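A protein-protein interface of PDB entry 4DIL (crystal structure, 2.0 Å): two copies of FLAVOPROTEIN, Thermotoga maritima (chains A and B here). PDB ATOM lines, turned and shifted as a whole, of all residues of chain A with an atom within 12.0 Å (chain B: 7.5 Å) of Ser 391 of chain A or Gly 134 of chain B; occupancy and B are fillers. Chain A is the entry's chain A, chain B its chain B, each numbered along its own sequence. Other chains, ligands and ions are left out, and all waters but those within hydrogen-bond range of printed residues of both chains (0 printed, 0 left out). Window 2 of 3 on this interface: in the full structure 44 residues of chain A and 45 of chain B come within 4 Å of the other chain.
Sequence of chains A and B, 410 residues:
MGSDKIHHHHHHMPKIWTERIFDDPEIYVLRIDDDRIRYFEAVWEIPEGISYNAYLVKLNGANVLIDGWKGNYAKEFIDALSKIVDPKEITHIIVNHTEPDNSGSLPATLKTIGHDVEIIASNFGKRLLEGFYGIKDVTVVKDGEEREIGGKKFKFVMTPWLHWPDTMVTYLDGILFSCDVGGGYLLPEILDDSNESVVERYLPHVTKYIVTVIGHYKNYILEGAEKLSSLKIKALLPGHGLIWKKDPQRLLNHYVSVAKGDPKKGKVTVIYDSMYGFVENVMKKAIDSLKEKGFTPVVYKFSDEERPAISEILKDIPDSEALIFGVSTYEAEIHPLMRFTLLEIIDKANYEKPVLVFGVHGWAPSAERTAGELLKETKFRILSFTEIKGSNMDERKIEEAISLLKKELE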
ATOM      1  N   TYR A 276      -1.469  31.337   0.043  1.00  0.00           N
ATOM      2  CA  TYR A 276      -2.482  31.069   1.056  1.00  0.00           C
ATOM      3  C   TYR A 276      -2.596  29.589   1.384  1.00  0.00           C
ATOM      4  O   TYR A 276      -3.190  29.221   2.400  1.00  0.00           O
ATOM      5  CB  TYR A 276      -3.849  31.608   0.619  1.00  0.00           C
ATOM      6  CG  TYR A 276      -3.795  32.970  -0.033  1.00  0.00           C
ATOM      7  CD1 TYR A 276      -3.281  34.066   0.647  1.00  0.00           C
ATOM      8  CD2 TYR A 276      -4.267  33.158  -1.330  1.00  0.00           C
ATOM      9  CE1 TYR A 276      -3.231  35.311   0.056  1.00  0.00           C
ATOM     10  CE2 TYR A 276      -4.226  34.405  -1.932  1.00  0.00           C
ATOM     11  CZ  TYR A 276      -3.706  35.476  -1.233  1.00  0.00           C
ATOM     12  OH  TYR A 276      -3.659  36.716  -1.830  1.00  0.00           O
ATOM     13  N   GLY A 277      -2.039  28.748   0.519  1.00  0.00           N
ATOM     14  CA  GLY A 277      -2.061  27.315   0.735  1.00  0.00           C
ATOM     15  C   GLY A 277      -2.924  26.567  -0.258  1.00  0.00           C
ATOM     16  O   GLY A 277      -2.906  25.335  -0.293  1.00  0.00           O
ATOM     17  N   PHE A 278      -3.682  27.292  -1.076  1.00  0.00           N
ATOM     18  CA  PHE A 278      -4.543  26.625  -2.060  1.00  0.00           C
ATOM     19  C   PHE A 278      -3.702  25.926  -3.129  1.00  0.00           C
ATOM     20  O   PHE A 278      -3.990  24.798  -3.531  1.00  0.00           O
ATOM     21  CB  PHE A 278      -5.525  27.610  -2.703  1.00  0.00           C
ATOM     22  CG  PHE A 278      -6.534  28.179  -1.743  1.00  0.00           C
ATOM     23  CD1 PHE A 278      -7.582  27.398  -1.267  1.00  0.00           C
ATOM     24  CD2 PHE A 278      -6.440  29.498  -1.322  1.00  0.00           C
ATOM     25  CE1 PHE A 278      -8.517  27.919  -0.380  1.00  0.00           C
ATOM     26  CE2 PHE A 278      -7.370  30.034  -0.439  1.00  0.00           C
ATOM     27  CZ  PHE A 278      -8.415  29.245   0.032  1.00  0.00           C
ATOM     28  N   VAL A 279      -2.664  26.610  -3.596  1.00  0.00           N
ATOM     29  CA  VAL A 279      -1.719  25.994  -4.516  1.00  0.00           C
ATOM     30  C   VAL A 279      -0.956  24.864  -3.828  1.00  0.00           C
ATOM     31  O   VAL A 279      -0.834  23.775  -4.382  1.00  0.00           O
ATOM     32  CB  VAL A 279      -0.747  27.023  -5.115  1.00  0.00           C
ATOM     33  CG1 VAL A 279       0.445  26.328  -5.730  1.00  0.00           C
ATOM     34  CG2 VAL A 279      -1.461  27.888  -6.155  1.00  0.00           C
ATOM     35  N   GLU A 280      -0.465  25.120  -2.618  1.00  0.00           N
ATOM     36  CA  GLU A 280       0.278  24.107  -1.862  1.00  0.00           C
ATOM     37  C   GLU A 280      -0.488  22.788  -1.757  1.00  0.00           C
ATOM     38  O   GLU A 280       0.087  21.717  -1.936  1.00  0.00           O
ATOM     39  CB  GLU A 280       0.643  24.623  -0.466  1.00  0.00           C
ATOM     40  CG  GLU A 280       1.122  23.552   0.510  1.00  0.00           C
ATOM     41  CD  GLU A 280       2.499  22.963   0.169  1.00  0.00           C
ATOM     42  OE1 GLU A 280       3.223  23.528  -0.688  1.00  0.00           O
ATOM     43  OE2 GLU A 280       2.859  21.925   0.772  1.00  0.00           O
ATOM     44  N   ASN A 281      -1.789  22.866  -1.498  1.00  0.00           N
ATOM     45  CA  ASN A 281      -2.599  21.656  -1.346  1.00  0.00           C
ATOM     46  C   ASN A 281      -2.710  20.843  -2.632  1.00  0.00           C
ATOM     47  O   ASN A 281      -2.636  19.616  -2.600  1.00  0.00           O
ATOM     48  CB  ASN A 281      -3.982  21.986  -0.769  1.00  0.00           C
ATOM     49  CG  ASN A 281      -3.900  22.561   0.637  1.00  0.00           C
ATOM     50  OD1 ASN A 281      -2.855  22.472   1.295  1.00  0.00           O
ATOM     51  ND2 ASN A 281      -5.001  23.149   1.111  1.00  0.00           N
ATOM     52  N   VAL A 282      -2.877  21.520  -3.764  1.00  0.00           N
ATOM     53  CA  VAL A 282      -2.869  20.831  -5.052  1.00  0.00           C
ATOM     54  C   VAL A 282      -1.479  20.251  -5.353  1.00  0.00           C
ATOM     55  O   VAL A 282      -1.353  19.095  -5.753  1.00  0.00           O
ATOM     56  CB  VAL A 282      -3.332  21.755  -6.197  1.00  0.00           C
ATOM     57  CG1 VAL A 282      -2.965  21.174  -7.547  1.00  0.00           C
ATOM     58  CG2 VAL A 282      -4.828  21.986  -6.113  1.00  0.00           C
ATOM     59  N   LYS A 285      -0.346  17.141  -3.430  1.00  0.00           N
ATOM     60  CA  LYS A 285      -0.946  15.927  -3.978  1.00  0.00           C
ATOM     61  C   LYS A 285      -0.310  15.502  -5.291  1.00  0.00           C
ATOM     62  O   LYS A 285      -0.186  14.308  -5.567  1.00  0.00           O
ATOM     63  CB  LYS A 285      -2.452  16.095  -4.177  1.00  0.00           C
ATOM     64  CG  LYS A 285      -3.229  16.271  -2.889  1.00  0.00           C
ATOM     65  CD  LYS A 285      -4.704  16.480  -3.188  1.00  0.00           C
ATOM     66  CE  LYS A 285      -5.485  16.884  -1.944  1.00  0.00           C
ATOM     67  NZ  LYS A 285      -6.821  17.461  -2.298  1.00  0.00           N
ATOM     68  N   GLY A 359      -2.735  25.874 -12.518  1.00  0.00           N
ATOM     69  CA  GLY A 359      -2.923  27.299 -12.298  1.00  0.00           C
ATOM     70  C   GLY A 359      -4.222  27.687 -11.609  1.00  0.00           C
ATOM     71  O   GLY A 359      -5.215  26.965 -11.682  1.00  0.00           O
ATOM     72  N   VAL A 360      -4.198  28.822 -10.918  1.00  0.00           N
ATOM     73  CA  VAL A 360      -5.425  29.423 -10.378  1.00  0.00           C
ATOM     74  C   VAL A 360      -6.011  30.372 -11.416  1.00  0.00           C
ATOM     75  O   VAL A 360      -5.271  31.056 -12.131  1.00  0.00           O
ATOM     76  CB  VAL A 360      -5.156  30.223  -9.100  1.00  0.00           C
ATOM     77  CG1 VAL A 360      -6.467  30.735  -8.503  1.00  0.00           C
ATOM     78  CG2 VAL A 360      -4.423  29.364  -8.098  1.00  0.00           C
ATOM     79  N   HIS A 361      -7.337  30.403 -11.515  1.00  0.00           N
ATOM     80  CA  HIS A 361      -8.011  31.346 -12.399  1.00  0.00           C
ATOM     81  C   HIS A 361      -7.964  32.719 -11.732  1.00  0.00           C
ATOM     82  O   HIS A 361      -8.159  32.833 -10.519  1.00  0.00           O
ATOM     83  CB  HIS A 361      -9.463  30.900 -12.638  1.00  0.00           C
ATOM     84  CG  HIS A 361     -10.129  31.535 -13.813  1.00  0.00           C
ATOM     85  ND1 HIS A 361      -9.503  32.498 -14.607  1.00  0.00           N
ATOM     86  CD2 HIS A 361     -11.357  31.368 -14.349  1.00  0.00           C
ATOM     87  CE1 HIS A 361     -10.327  32.874 -15.555  1.00  0.00           C
ATOM     88  NE2 HIS A 361     -11.462  32.208 -15.434  1.00  0.00           N
ATOM     89  N   GLU A 387      -6.752  23.490 -13.671  1.00  0.00           N
ATOM     90  CA  GLU A 387      -7.141  24.600 -12.810  1.00  0.00           C
ATOM     91  C   GLU A 387      -7.032  24.275 -11.319  1.00  0.00           C
ATOM     92  O   GLU A 387      -7.662  23.339 -10.824  1.00  0.00           O
ATOM     93  CB  GLU A 387      -8.561  25.079 -13.122  1.00  0.00           C
ATOM     94  CG  GLU A 387      -8.976  26.283 -12.278  1.00  0.00           C
ATOM     95  CD  GLU A 387     -10.358  26.788 -12.633  1.00  0.00           C
ATOM     96  OE1 GLU A 387     -10.939  26.274 -13.618  1.00  0.00           O
ATOM     97  OE2 GLU A 387     -10.857  27.697 -11.929  1.00  0.00           O
ATOM     98  N   ILE A 388      -6.236  25.065 -10.606  1.00  0.00           N
ATOM     99  CA  ILE A 388      -6.188  24.992  -9.150  1.00  0.00           C
ATOM    100  C   ILE A 388      -7.381  25.755  -8.575  1.00  0.00           C
ATOM    101  O   ILE A 388      -7.444  26.987  -8.664  1.00  0.00           O
ATOM    102  CB  ILE A 388      -4.883  25.602  -8.597  1.00  0.00           C
ATOM    103  CG1 ILE A 388      -3.687  24.738  -8.983  1.00  0.00           C
ATOM    104  CG2 ILE A 388      -4.939  25.735  -7.080  1.00  0.00           C
ATOM    105  CD1 ILE A 388      -2.370  25.440  -8.768  1.00  0.00           C
ATOM    106  N   LYS A 389      -8.330  25.022  -8.002  1.00  0.00           N
ATOM    107  CA  LYS A 389      -9.469  25.636  -7.329  1.00  0.00           C
ATOM    108  C   LYS A 389      -9.262  25.569  -5.826  1.00  0.00           C
ATOM    109  O   LYS A 389      -8.334  24.909  -5.352  1.00  0.00           O
ATOM    110  CB  LYS A 389     -10.771  24.918  -7.695  1.00  0.00           C
ATOM    111  CG  LYS A 389     -11.130  24.960  -9.167  1.00  0.00           C
ATOM    112  CD  LYS A 389     -12.541  24.437  -9.394  1.00  0.00           C
ATOM    113  CE  LYS A 389     -13.023  24.759 -10.798  1.00  0.00           C
ATOM    114  NZ  LYS A 389     -13.236  23.535 -11.623  1.00  0.00           N
ATOM    115  N   GLY A 390     -10.123  26.258  -5.084  1.00  0.00           N
ATOM    116  CA  GLY A 390     -10.119  26.158  -3.639  1.00  0.00           C
ATOM    117  C   GLY A 390     -11.015  25.026  -3.170  1.00  0.00           C
ATOM    118  O   GLY A 390     -10.638  23.851  -3.228  1.00  0.00           O
ATOM    119  N   SER A 391     -12.219  25.389  -2.735  1.00  0.00           N
ATOM    120  CA  SER A 391     -13.154  24.461  -2.093  1.00  0.00           C
ATOM    121  C   SER A 391     -13.675  23.310  -2.960  1.00  0.00           C
ATOM    122  O   SER A 391     -13.721  22.160  -2.509  1.00  0.00           O
ATOM    123  CB  SER A 391     -14.345  25.240  -1.526  1.00  0.00           C
ATOM    124  OG  SER A 391     -14.362  25.152  -0.116  1.00  0.00           O
ATOM    125  N   ASN A 392     -14.087  23.624  -4.186  1.00  0.00           N
ATOM    126  CA  ASN A 392     -14.689  22.630  -5.069  1.00  0.00           C
ATOM    127  C   ASN A 392     -13.671  21.851  -5.910  1.00  0.00           C
ATOM    128  O   ASN A 392     -14.051  21.177  -6.877  1.00  0.00           O
ATOM    129  CB  ASN A 392     -15.699  23.306  -5.994  1.00  0.00           C
ATOM    130  CG  ASN A 392     -15.163  24.593  -6.593  1.00  0.00           C
ATOM    131  OD1 ASN A 392     -14.060  25.034  -6.258  1.00  0.00           O
ATOM    132  ND2 ASN A 392     -15.940  25.202  -7.489  1.00  0.00           N
ATOM    133  N   MET A 393     -12.392  21.954  -5.541  1.00  0.00           N
ATOM    134  CA  MET A 393     -11.298  21.315  -6.277  1.00  0.00           C
ATOM    135  C   MET A 393     -11.507  19.813  -6.381  1.00  0.00           C
ATOM    136  O   MET A 393     -11.615  19.123  -5.362  1.00  0.00           O
ATOM    137  CB  MET A 393      -9.948  21.585  -5.596  1.00  0.00           C
ATOM    138  CG  MET A 393      -8.754  20.943  -6.309  1.00  0.00           C
ATOM    139  SD  MET A 393      -8.512  21.642  -7.956  1.00  0.00           S
ATOM    140  CE  MET A 393      -7.319  20.484  -8.637  1.00  0.00           C
ATOM    141  N   ASP A 394     -11.563  19.314  -7.613  1.00  0.00           N
ATOM    142  CA  ASP A 394     -11.623  17.875  -7.851  1.00  0.00           C
ATOM    143  C   ASP A 394     -10.216  17.303  -8.019  1.00  0.00           C
ATOM    144  O   ASP A 394      -9.582  17.476  -9.062  1.00  0.00           O
ATOM    145  CB  ASP A 394     -12.486  17.559  -9.079  1.00  0.00           C
ATOM    146  CG  ASP A 394     -12.655  16.063  -9.307  1.00  0.00           C
ATOM    147  OD1 ASP A 394     -12.293  15.277  -8.400  1.00  0.00           O
ATOM    148  OD2 ASP A 394     -13.151  15.675 -10.391  1.00  0.00           O
ATOM    149  N   GLU A 395      -9.743  16.619  -6.980  1.00  0.00           N
ATOM    150  CA  GLU A 395      -8.416  16.000  -6.964  1.00  0.00           C
ATOM    151  C   GLU A 395      -8.207  14.952  -8.069  1.00  0.00           C
ATOM    152  O   GLU A 395      -7.082  14.696  -8.480  1.00  0.00           O
ATOM    153  CB  GLU A 395      -8.155  15.408  -5.571  1.00  0.00           C
ATOM    154  CG  GLU A 395      -7.152  14.270  -5.512  1.00  0.00           C
ATOM    155  CD  GLU A 395      -7.642  13.130  -4.637  1.00  0.00           C
ATOM    156  OE1 GLU A 395      -8.095  13.414  -3.500  1.00  0.00           O
ATOM    157  OE2 GLU A 395      -7.598  11.960  -5.093  1.00  0.00           O
ATOM    158  N   ARG A 396      -9.293  14.369  -8.570  1.00  0.00           N
ATOM    159  CA  ARG A 396      -9.206  13.436  -9.700  1.00  0.00           C
ATOM    160  C   ARG A 396      -8.397  14.002 -10.866  1.00  0.00           C
ATOM    161  O   ARG A 396      -7.701  13.267 -11.568  1.00  0.00           O
ATOM    162  CB  ARG A 396     -10.602  13.064 -10.204  1.00  0.00           C
ATOM    163  CG  ARG A 396     -11.133  11.738  -9.688  1.00  0.00           C
ATOM    164  CD  ARG A 396     -12.475  11.398 -10.336  1.00  0.00           C
ATOM    165  NE  ARG A 396     -13.458  12.471 -10.174  1.00  0.00           N
ATOM    166  CZ  ARG A 396     -14.185  12.981 -11.167  1.00  0.00           C
ATOM    167  NH1 ARG A 396     -14.049  12.516 -12.406  1.00  0.00           N
ATOM    168  NH2 ARG A 396     -15.053  13.953 -10.922  1.00  0.00           N
ATOM    169  N   ILE A 398      -5.966  16.171 -10.743  1.00  0.00           N
ATOM    170  CA  ILE A 398      -4.546  16.135 -10.411  1.00  0.00           C
ATOM    171  C   ILE A 398      -3.961  14.774 -10.791  1.00  0.00           C
ATOM    172  O   ILE A 398      -2.960  14.688 -11.508  1.00  0.00           O
ATOM    173  CB  ILE A 398      -4.301  16.391  -8.912  1.00  0.00           C
ATOM    174  CG1 ILE A 398      -4.905  17.732  -8.481  1.00  0.00           C
ATOM    175  CG2 ILE A 398      -2.807  16.353  -8.599  1.00  0.00           C
ATOM    176  CD1 ILE A 398      -4.855  17.987  -6.972  1.00  0.00           C
ATOM    177  N   PRO B 107     -13.367  30.184   9.048  1.00  0.00           N
ATOM    178  CA  PRO B 107     -14.048  28.892   9.205  1.00  0.00           C
ATOM    179  C   PRO B 107     -13.902  28.311  10.608  1.00  0.00           C
ATOM    180  O   PRO B 107     -14.853  27.735  11.130  1.00  0.00           O
ATOM    181  CB  PRO B 107     -13.335  27.989   8.195  1.00  0.00           C
ATOM    182  CG  PRO B 107     -12.765  28.917   7.182  1.00  0.00           C
ATOM    183  CD  PRO B 107     -12.354  30.133   7.975  1.00  0.00           C
ATOM    184  N   ARG B 127     -18.872  35.782  -3.266  1.00  0.00           N
ATOM    185  CA  ARG B 127     -18.420  34.780  -4.229  1.00  0.00           C
ATOM    186  C   ARG B 127     -17.072  34.203  -3.825  1.00  0.00           C
ATOM    187  O   ARG B 127     -16.837  33.004  -3.968  1.00  0.00           O
ATOM    188  CB  ARG B 127     -18.344  35.384  -5.634  1.00  0.00           C
ATOM    189  CG  ARG B 127     -19.645  36.026  -6.083  1.00  0.00           C
ATOM    190  CD  ARG B 127     -19.436  36.919  -7.290  1.00  0.00           C
ATOM    191  NE  ARG B 127     -18.755  36.205  -8.366  1.00  0.00           N
ATOM    192  CZ  ARG B 127     -18.601  36.674  -9.602  1.00  0.00           C
ATOM    193  NH1 ARG B 127     -19.092  37.864  -9.930  1.00  0.00           N
ATOM    194  NH2 ARG B 127     -17.959  35.950 -10.511  1.00  0.00           N
ATOM    195  N   LEU B 128     -16.194  35.056  -3.300  1.00  0.00           N
ATOM    196  CA  LEU B 128     -14.856  34.614  -2.891  1.00  0.00           C
ATOM    197  C   LEU B 128     -14.876  33.764  -1.620  1.00  0.00           C
ATOM    198  O   LEU B 128     -14.075  32.856  -1.464  1.00  0.00           O
ATOM    199  CB  LEU B 128     -13.921  35.812  -2.720  1.00  0.00           C
ATOM    200  CG  LEU B 128     -13.508  36.470  -4.041  1.00  0.00           C
ATOM    201  CD1 LEU B 128     -12.767  37.794  -3.827  1.00  0.00           C
ATOM    202  CD2 LEU B 128     -12.663  35.485  -4.852  1.00  0.00           C
ATOM    203  N   LEU B 129     -15.797  34.067  -0.709  1.00  0.00           N
ATOM    204  CA  LEU B 129     -15.917  33.293   0.522  1.00  0.00           C
ATOM    205  C   LEU B 129     -16.342  31.865   0.194  1.00  0.00           C
ATOM    206  O   LEU B 129     -15.991  30.921   0.899  1.00  0.00           O
ATOM    207  CB  LEU B 129     -16.904  33.957   1.487  1.00  0.00           C
ATOM    208  CG  LEU B 129     -16.401  35.192   2.230  1.00  0.00           C
ATOM    209  CD1 LEU B 129     -17.537  35.864   2.995  1.00  0.00           C
ATOM    210  CD2 LEU B 129     -15.300  34.790   3.183  1.00  0.00           C
ATOM    211  N   GLU B 130     -17.092  31.713  -0.895  1.00  0.00           N
ATOM    212  CA  GLU B 130     -17.507  30.395  -1.348  1.00  0.00           C
ATOM    213  C   GLU B 130     -16.346  29.693  -2.031  1.00  0.00           C
ATOM    214  O   GLU B 130     -16.087  28.519  -1.776  1.00  0.00           O
ATOM    215  CB  GLU B 130     -18.705  30.479  -2.308  1.00  0.00           C
ATOM    216  CG  GLU B 130     -19.267  29.101  -2.660  1.00  0.00           C
ATOM    217  CD  GLU B 130     -20.280  29.131  -3.794  1.00  0.00           C
ATOM    218  OE1 GLU B 130     -20.029  28.461  -4.822  1.00  0.00           O
ATOM    219  OE2 GLU B 130     -21.327  29.805  -3.653  1.00  0.00           O
ATOM    220  N   GLY B 131     -15.649  30.427  -2.898  1.00  0.00           N
ATOM    221  CA  GLY B 131     -14.472  29.922  -3.581  1.00  0.00           C
ATOM    222  C   GLY B 131     -13.347  29.473  -2.662  1.00  0.00           C
ATOM    223  O   GLY B 131     -12.766  28.401  -2.851  1.00  0.00           O
ATOM    224  N   PHE B 132     -13.025  30.291  -1.668  1.00  0.00           N
ATOM    225  CA  PHE B 132     -11.970  29.944  -0.723  1.00  0.00           C
ATOM    226  C   PHE B 132     -12.413  28.878   0.266  1.00  0.00           C
ATOM    227  O   PHE B 132     -11.719  27.883   0.466  1.00  0.00           O
ATOM    228  CB  PHE B 132     -11.516  31.178   0.063  1.00  0.00           C
ATOM    229  CG  PHE B 132     -10.812  32.206  -0.766  1.00  0.00           C
ATOM    230  CD1 PHE B 132     -10.037  31.832  -1.857  1.00  0.00           C
ATOM    231  CD2 PHE B 132     -10.915  33.556  -0.445  1.00  0.00           C
ATOM    232  CE1 PHE B 132      -9.382  32.795  -2.623  1.00  0.00           C
ATOM    233  CE2 PHE B 132     -10.269  34.521  -1.201  1.00  0.00           C
ATOM    234  CZ  PHE B 132      -9.505  34.141  -2.294  1.00  0.00           C
ATOM    235  N   TYR B 133     -13.568  29.095   0.892  1.00  0.00           N
ATOM    236  CA  TYR B 133     -13.919  28.327   2.080  1.00  0.00           C
ATOM    237  C   TYR B 133     -15.178  27.456   1.974  1.00  0.00           C
ATOM    238  O   TYR B 133     -15.473  26.676   2.889  1.00  0.00           O
ATOM    239  CB  TYR B 133     -14.051  29.270   3.279  1.00  0.00           C
ATOM    240  CG  TYR B 133     -12.889  30.232   3.457  1.00  0.00           C
ATOM    241  CD1 TYR B 133     -11.616  29.767   3.771  1.00  0.00           C
ATOM    242  CD2 TYR B 133     -13.074  31.607   3.335  1.00  0.00           C
ATOM    243  CE1 TYR B 133     -10.552  30.644   3.949  1.00  0.00           C
ATOM    244  CE2 TYR B 133     -12.022  32.492   3.515  1.00  0.00           C
ATOM    245  CZ  TYR B 133     -10.761  32.001   3.817  1.00  0.00           C
ATOM    246  OH  TYR B 133      -9.710  32.878   3.989  1.00  0.00           O
ATOM    247  N   GLY B 134     -15.913  27.589   0.873  1.00  0.00           N
ATOM    248  CA  GLY B 134     -17.172  26.880   0.716  1.00  0.00           C
ATOM    249  C   GLY B 134     -18.274  27.491   1.569  1.00  0.00           C
ATOM    250  O   GLY B 134     -19.277  26.850   1.878  1.00  0.00           O
ATOM    251  N   ILE B 135     -18.079  28.742   1.964  1.00  0.00           N
ATOM    252  CA  ILE B 135     -19.076  29.457   2.749  1.00  0.00           C
ATOM    253  C   ILE B 135     -20.121  30.062   1.807  1.00  0.00           C
ATOM    254  O   ILE B 135     -19.786  30.815   0.893  1.00  0.00           O
ATOM    255  CB  ILE B 135     -18.423  30.526   3.643  1.00  0.00           C
ATOM    256  CG1 ILE B 135     -17.528  29.852   4.678  1.00  0.00           C
ATOM    257  CG2 ILE B 135     -19.468  31.333   4.377  1.00  0.00           C
ATOM    258  CD1 ILE B 135     -16.702  30.827   5.500  1.00  0.00           C
ATOM    259  N   LYS B 136     -21.386  29.720   2.040  1.00  0.00           N
ATOM    260  CA  LYS B 136     -22.452  29.955   1.068  1.00  0.00           C
ATOM    261  C   LYS B 136     -23.527  30.919   1.545  1.00  0.00           C
ATOM    262  O   LYS B 136     -24.112  31.656   0.745  1.00  0.00           O
ATOM    263  CB  LYS B 136     -23.107  28.621   0.700  1.00  0.00           C
ATOM    264  CG  LYS B 136     -22.510  27.950  -0.520  1.00  0.00           C
ATOM    265  CD  LYS B 136     -22.722  26.443  -0.492  1.00  0.00           C
ATOM    266  CE  LYS B 136     -22.117  25.783  -1.725  1.00  0.00           C
ATOM    267  NZ  LYS B 136     -22.910  26.090  -2.956  1.00  0.00           N
ATOM    268  N   ASP B 137     -23.801  30.908   2.841  1.00  0.00           N
ATOM    269  CA  ASP B 137     -24.874  31.746   3.349  1.00  0.00           C
ATOM    270  C   ASP B 137     -24.351  33.089   3.854  1.00  0.00           C
ATOM    271  O   ASP B 137     -24.070  33.271   5.040  1.00  0.00           O
ATOM    272  CB  ASP B 137     -25.714  30.997   4.392  1.00  0.00           C
ATOM    273  CG  ASP B 137     -26.609  29.927   3.759  1.00  0.00           C
ATOM    274  OD1 ASP B 137     -27.316  30.241   2.770  1.00  0.00           O
ATOM    275  OD2 ASP B 137     -26.593  28.771   4.241  1.00  0.00           O
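N of Ser 391 of chain A lies within hydrogen-bond range of O of Gly 131 of chain B, at 3.1 Å.
The backbone NH (N) of Gly 134 of chain B sits at hydrogen-bond distance from the side-chain hydroxyl (OG) of Ser 391 of chain A.
O of Leu 129 of chain B lies within hydrogen-bond range of N of Gly 134 of chain B, at 3.3 Å.
The backbone NH (N) of Glu 130 of chain B sits close to the backbone carbonyl oxygen (O) of Ile 135 of chain B.
Among the printed residues, pairs that only touch across the chains: Ser 391 of chain A with Tyr 133 of chain B (3.2 Å), Phe 278 of chain A with Phe 132 of chain B (3.3 Å), Gly 390 of chain A with Gly 131 of chain B (3.6 Å), Ser 391 of chain A with Glu 130 of chain B (3.7 Å) and Ser 391 of chain A with Phe 132 of chain B (3.8 Å).
Of the printed residues of chain B, Phe 278 of chain A touches Phe 132 (3.3 Å).
Ser 391 of chain A touches just these residues of chain B: Glu 130 (3.7 Å), Gly 131 (3.1 Å), Phe 132 (3.8 Å), Tyr 133 (3.2 Å) and Gly 134 (3.1 Å).
Of the printed residues of chain A, Phe 132 of chain B touches Phe 278 and Ser 391.
Printed residues of chain A within 4 Å of Tyr 133 of chain B: Ser 391.
Gly 134 of chain B touches one residue of chain A.
Ile 135 of chain B touches none of the printed residues of chain A.
No residue of chain A comes within 4 Å of Lys 136 of chain B.
Of the 22 printed residues of chain A, 3 touch a printed residue of chain B.
Among the printed residues, 7 pairs touch across the chains.
No position is printed for both chains.
Of the 7 pairs that touch across the chains among the printed residues, none has its exchanged pair printed and touching as well.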
